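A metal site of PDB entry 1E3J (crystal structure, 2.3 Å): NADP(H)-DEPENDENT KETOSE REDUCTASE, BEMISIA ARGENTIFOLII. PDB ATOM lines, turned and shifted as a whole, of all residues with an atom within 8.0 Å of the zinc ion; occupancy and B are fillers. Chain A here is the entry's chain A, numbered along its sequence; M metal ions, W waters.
The side-chain carboxylate of Asp 44 lies within hydrogen-bond range of the backbone NH of Cys 41 (3.2 Å). The side-chain carboxylate of Asp 44 lies within hydrogen-bond range of a ring nitrogen (ND1) of His 66 (3.3 Å). The side-chain carboxylate (OE1) of Glu 67 lies within salt-bridge range of the side-chain amino group (NZ) of Lys 344 (2.7 Å). The side-chain sulfur (SG) of Cys 41 sits close to the backbone NH (N) of Ser 43 (3.3 Å). The backbone carbonyl oxygen (O) of Glu 67 is in hydrogen-bond range of the backbone NH (N) of Gly 39 (2.7 Å). The side-chain carboxylate (OE2) of Glu 152 lies within hydrogen-bond range of the side-chain hydroxyl (OH) of Tyr 297 (2.7 Å).
Residues that only touch the zinc ion: Glu 152. Of the 19 residues printed, 4 come within 4 Å of the zinc ion. The nearest printed residue that does not touch the zinc ion is Asp 44 (4.7 Å).
The zinc ion is bound by water W1 (2.1 Å), NE2 of His 66 (2.2 Å), OE2 of Glu 67 (2.3 Å) and SG of Cys 41 (2.4 Å).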
ATOM      1  N   GLY A  39     -20.278  11.475 -13.337  1.00  0.00           N
ATOM      2  CA  GLY A  39     -19.592  12.690 -13.709  1.00  0.00           C
ATOM      3  C   GLY A  39     -20.043  13.765 -12.748  1.00  0.00           C
ATOM      4  O   GLY A  39     -21.062  13.626 -12.084  1.00  0.00           O
ATOM      5  N   ILE A  40     -19.282  14.839 -12.649  1.00  0.00           N
ATOM      6  CA  ILE A  40     -19.694  15.894 -11.752  1.00  0.00           C
ATOM      7  C   ILE A  40     -19.685  17.210 -12.497  1.00  0.00           C
ATOM      8  O   ILE A  40     -18.934  17.362 -13.454  1.00  0.00           O
ATOM      9  CB  ILE A  40     -18.793  15.949 -10.519  1.00  0.00           C
ATOM     10  CG1 ILE A  40     -17.328  16.109 -10.925  1.00  0.00           C
ATOM     11  CG2 ILE A  40     -18.975  14.671  -9.720  1.00  0.00           C
ATOM     12  CD1 ILE A  40     -16.349  16.079  -9.715  1.00  0.00           C
ATOM     13  N   CYS A  41     -20.542  18.151 -12.085  1.00  0.00           N
ATOM     14  CA  CYS A  41     -20.586  19.432 -12.760  1.00  0.00           C
ATOM     15  C   CYS A  41     -20.601  20.579 -11.770  1.00  0.00           C
ATOM     16  O   CYS A  41     -20.534  20.378 -10.553  1.00  0.00           O
ATOM     17  CB  CYS A  41     -21.810  19.491 -13.685  1.00  0.00           C
ATOM     18  SG  CYS A  41     -23.390  19.855 -12.870  1.00  0.00           S
ATOM     19  N   GLY A  42     -20.689  21.800 -12.303  1.00  0.00           N
ATOM     20  CA  GLY A  42     -20.685  22.978 -11.453  1.00  0.00           C
ATOM     21  C   GLY A  42     -21.760  22.939 -10.380  1.00  0.00           C
ATOM     22  O   GLY A  42     -21.570  23.397  -9.243  1.00  0.00           O
ATOM     23  N   SER A  43     -22.901  22.369 -10.750  1.00  0.00           N
ATOM     24  CA  SER A  43     -24.012  22.251  -9.819  1.00  0.00           C
ATOM     25  C   SER A  43     -23.623  21.445  -8.585  1.00  0.00           C
ATOM     26  O   SER A  43     -23.972  21.829  -7.474  1.00  0.00           O
ATOM     27  CB  SER A  43     -25.213  21.650 -10.525  1.00  0.00           C
ATOM     28  OG  SER A  43     -26.219  21.340  -9.586  1.00  0.00           O
ATOM     29  N   ASP A  44     -22.918  20.327  -8.764  1.00  0.00           N
ATOM     30  CA  ASP A  44     -22.482  19.537  -7.590  1.00  0.00           C
ATOM     31  C   ASP A  44     -21.482  20.381  -6.797  1.00  0.00           C
ATOM     32  O   ASP A  44     -21.559  20.494  -5.572  1.00  0.00           O
ATOM     33  CB  ASP A  44     -21.777  18.227  -7.987  1.00  0.00           C
ATOM     34  CG  ASP A  44     -22.703  17.211  -8.643  1.00  0.00           C
ATOM     35  OD1 ASP A  44     -23.736  16.782  -8.019  1.00  0.00           O
ATOM     36  OD2 ASP A  44     -22.381  16.816  -9.790  1.00  0.00           O
ATOM     37  N   GLY A  65     -24.180  13.452  -6.545  1.00  0.00           N
ATOM     38  CA  GLY A  65     -24.079  12.752  -7.813  1.00  0.00           C
ATOM     39  C   GLY A  65     -25.347  12.618  -8.651  1.00  0.00           C
ATOM     40  O   GLY A  65     -26.363  12.155  -8.143  1.00  0.00           O
ATOM     41  N   HIS A  66     -25.294  13.007  -9.927  1.00  0.00           N
ATOM     42  CA  HIS A  66     -26.438  12.850 -10.812  1.00  0.00           C
ATOM     43  C   HIS A  66     -26.138  12.556 -12.303  1.00  0.00           C
ATOM     44  O   HIS A  66     -27.057  12.515 -13.129  1.00  0.00           O
ATOM     45  CB  HIS A  66     -27.347  14.079 -10.688  1.00  0.00           C
ATOM     46  CG  HIS A  66     -26.692  15.350 -11.134  1.00  0.00           C
ATOM     47  ND1 HIS A  66     -26.056  16.201 -10.261  1.00  0.00           N
ATOM     48  CD2 HIS A  66     -26.452  15.841 -12.375  1.00  0.00           C
ATOM     49  CE1 HIS A  66     -25.449  17.159 -10.935  1.00  0.00           C
ATOM     50  NE2 HIS A  66     -25.675  16.957 -12.216  1.00  0.00           N
ATOM     51  N   GLU A  67     -24.890  12.377 -12.690  1.00  0.00           N
ATOM     52  CA  GLU A  67     -24.568  12.096 -14.092  1.00  0.00           C
ATOM     53  C   GLU A  67     -23.974  10.711 -14.058  1.00  0.00           C
ATOM     54  O   GLU A  67     -22.750  10.555 -13.992  1.00  0.00           O
ATOM     55  CB  GLU A  67     -23.523  13.064 -14.631  1.00  0.00           C
ATOM     56  CG  GLU A  67     -23.911  14.533 -14.466  1.00  0.00           C
ATOM     57  CD  GLU A  67     -22.853  15.476 -15.075  1.00  0.00           C
ATOM     58  OE1 GLU A  67     -21.809  14.987 -15.559  1.00  0.00           O
ATOM     59  OE2 GLU A  67     -23.092  16.706 -15.062  1.00  0.00           O
ATOM     60  N   PRO A  92     -31.478  11.094 -14.343  1.00  0.00           N
ATOM     61  CA  PRO A  92     -31.739  11.516 -12.964  1.00  0.00           C
ATOM     62  C   PRO A  92     -33.038  12.166 -12.515  1.00  0.00           C
ATOM     63  O   PRO A  92     -33.307  12.187 -11.315  1.00  0.00           O
ATOM     64  CB  PRO A  92     -30.521  12.407 -12.628  1.00  0.00           C
ATOM     65  CG  PRO A  92     -30.163  13.000 -13.984  1.00  0.00           C
ATOM     66  CD  PRO A  92     -30.351  11.851 -14.954  1.00  0.00           C
ATOM     67  N   PHE A 115     -35.069  15.138  -8.428  1.00  0.00           N
ATOM     68  CA  PHE A 115     -33.822  15.082  -9.203  1.00  0.00           C
ATOM     69  C   PHE A 115     -32.624  14.661  -8.312  1.00  0.00           C
ATOM     70  O   PHE A 115     -32.364  15.293  -7.262  1.00  0.00           O
ATOM     71  CB  PHE A 115     -33.574  16.443  -9.840  1.00  0.00           C
ATOM     72  CG  PHE A 115     -32.554  16.413 -10.908  1.00  0.00           C
ATOM     73  CD1 PHE A 115     -31.180  16.529 -10.600  1.00  0.00           C
ATOM     74  CD2 PHE A 115     -32.934  16.232 -12.237  1.00  0.00           C
ATOM     75  CE1 PHE A 115     -30.214  16.458 -11.590  1.00  0.00           C
ATOM     76  CE2 PHE A 115     -31.999  16.156 -13.247  1.00  0.00           C
ATOM     77  CZ  PHE A 115     -30.612  16.274 -12.936  1.00  0.00           C
ATOM     78  N   CYS A 116     -31.903  13.588  -8.699  1.00  0.00           N
ATOM     79  CA  CYS A 116     -30.732  13.085  -7.953  1.00  0.00           C
ATOM     80  C   CYS A 116     -29.750  14.182  -7.510  1.00  0.00           C
ATOM     81  O   CYS A 116     -29.184  14.885  -8.363  1.00  0.00           O
ATOM     82  CB  CYS A 116     -29.903  12.098  -8.800  1.00  0.00           C
ATOM     83  SG  CYS A 116     -30.720  10.549  -9.231  1.00  0.00           S
ATOM     84  N   GLU A 152     -25.943  12.341 -19.763  1.00  0.00           N
ATOM     85  CA  GLU A 152     -26.663  13.332 -18.981  1.00  0.00           C
ATOM     86  C   GLU A 152     -26.284  14.719 -19.497  1.00  0.00           C
ATOM     87  O   GLU A 152     -27.169  15.507 -19.800  1.00  0.00           O
ATOM     88  CB  GLU A 152     -26.358  13.177 -17.478  1.00  0.00           C
ATOM     89  CG  GLU A 152     -27.307  13.939 -16.512  1.00  0.00           C
ATOM     90  CD  GLU A 152     -27.040  15.446 -16.417  1.00  0.00           C
ATOM     91  OE1 GLU A 152     -25.931  15.916 -16.784  1.00  0.00           O
ATOM     92  OE2 GLU A 152     -27.916  16.177 -15.919  1.00  0.00           O
ATOM     93  N   PRO A 153     -24.979  15.064 -19.590  1.00  0.00           N
ATOM     94  CA  PRO A 153     -24.718  16.424 -20.112  1.00  0.00           C
ATOM     95  C   PRO A 153     -24.937  16.530 -21.634  1.00  0.00           C
ATOM     96  O   PRO A 153     -25.297  17.607 -22.150  1.00  0.00           O
ATOM     97  CB  PRO A 153     -23.256  16.716 -19.681  1.00  0.00           C
ATOM     98  CG  PRO A 153     -22.641  15.337 -19.513  1.00  0.00           C
ATOM     99  CD  PRO A 153     -23.805  14.532 -18.866  1.00  0.00           C
ATOM    100  N   VAL A 156     -28.440  17.613 -22.289  1.00  0.00           N
ATOM    101  CA  VAL A 156     -28.694  19.028 -22.091  1.00  0.00           C
ATOM    102  C   VAL A 156     -28.418  19.717 -23.416  1.00  0.00           C
ATOM    103  O   VAL A 156     -29.095  20.674 -23.798  1.00  0.00           O
ATOM    104  CB  VAL A 156     -27.745  19.680 -21.083  1.00  0.00           C
ATOM    105  CG1 VAL A 156     -28.015  21.180 -21.075  1.00  0.00           C
ATOM    106  CG2 VAL A 156     -27.939  19.074 -19.660  1.00  0.00           C
ATOM    107  N   ILE A 180     -20.597  22.299 -21.086  1.00  0.00           N
ATOM    108  CA  ILE A 180     -21.907  22.521 -21.684  1.00  0.00           C
ATOM    109  C   ILE A 180     -21.772  23.064 -23.123  1.00  0.00           C
ATOM    110  O   ILE A 180     -22.500  22.654 -24.022  1.00  0.00           O
ATOM    111  CB  ILE A 180     -22.770  23.482 -20.796  1.00  0.00           C
ATOM    112  CG1 ILE A 180     -22.973  22.817 -19.420  1.00  0.00           C
ATOM    113  CG2 ILE A 180     -24.164  23.707 -21.411  1.00  0.00           C
ATOM    114  CD1 ILE A 180     -23.500  21.369 -19.516  1.00  0.00           C
ATOM    115  N   ARG A 296     -32.438  21.322 -18.224  1.00  0.00           N
ATOM    116  CA  ARG A 296     -32.110  19.909 -18.260  1.00  0.00           C
ATOM    117  C   ARG A 296     -32.533  19.273 -19.571  1.00  0.00           C
ATOM    118  O   ARG A 296     -32.057  19.672 -20.610  1.00  0.00           O
ATOM    119  CB  ARG A 296     -32.773  19.184 -17.086  1.00  0.00           C
ATOM    120  CG  ARG A 296     -32.308  19.744 -15.742  1.00  0.00           C
ATOM    121  CD  ARG A 296     -32.773  18.904 -14.605  1.00  0.00           C
ATOM    122  NE  ARG A 296     -32.329  19.409 -13.320  1.00  0.00           N
ATOM    123  CZ  ARG A 296     -33.135  19.531 -12.264  1.00  0.00           C
ATOM    124  NH1 ARG A 296     -34.422  19.201 -12.363  1.00  0.00           N
ATOM    125  NH2 ARG A 296     -32.657  19.940 -11.091  1.00  0.00           N
ATOM    126  N   TYR A 297     -33.440  18.304 -19.521  1.00  0.00           N
ATOM    127  CA  TYR A 297     -33.843  17.550 -20.694  1.00  0.00           C
ATOM    128  C   TYR A 297     -35.211  16.898 -20.506  1.00  0.00           C
ATOM    129  O   TYR A 297     -35.702  16.716 -19.371  1.00  0.00           O
ATOM    130  CB  TYR A 297     -32.785  16.453 -20.994  1.00  0.00           C
ATOM    131  CG  TYR A 297     -32.105  15.963 -19.727  1.00  0.00           C
ATOM    132  CD1 TYR A 297     -32.807  15.202 -18.777  1.00  0.00           C
ATOM    133  CD2 TYR A 297     -30.800  16.394 -19.392  1.00  0.00           C
ATOM    134  CE1 TYR A 297     -32.236  14.921 -17.518  1.00  0.00           C
ATOM    135  CE2 TYR A 297     -30.250  16.122 -18.179  1.00  0.00           C
ATOM    136  CZ  TYR A 297     -30.957  15.402 -17.235  1.00  0.00           C
ATOM    137  OH  TYR A 297     -30.416  15.240 -16.000  1.00  0.00           O
ATOM    138  N   LYS A 344     -14.301  17.663 -18.204  1.00  0.00           N
ATOM    139  CA  LYS A 344     -15.208  16.893 -17.380  1.00  0.00           C
ATOM    140  C   LYS A 344     -14.462  15.954 -16.427  1.00  0.00           C
ATOM    141  O   LYS A 344     -13.575  15.200 -16.853  1.00  0.00           O
ATOM    142  CB  LYS A 344     -16.178  16.117 -18.296  1.00  0.00           C
ATOM    143  CG  LYS A 344     -17.067  15.108 -17.598  1.00  0.00           C
ATOM    144  CD  LYS A 344     -18.035  15.711 -16.555  1.00  0.00           C
ATOM    145  CE  LYS A 344     -19.108  16.621 -17.136  1.00  0.00           C
ATOM    146  NZ  LYS A 344     -20.064  16.989 -16.023  1.00  0.00           N
HETATM  147 ZN    ZN M   1     -24.530  17.898 -13.781  1.00  0.00          ZN
HETATM  148  O   HOH W   1     -25.669  18.565 -15.470  1.00  0.00           O
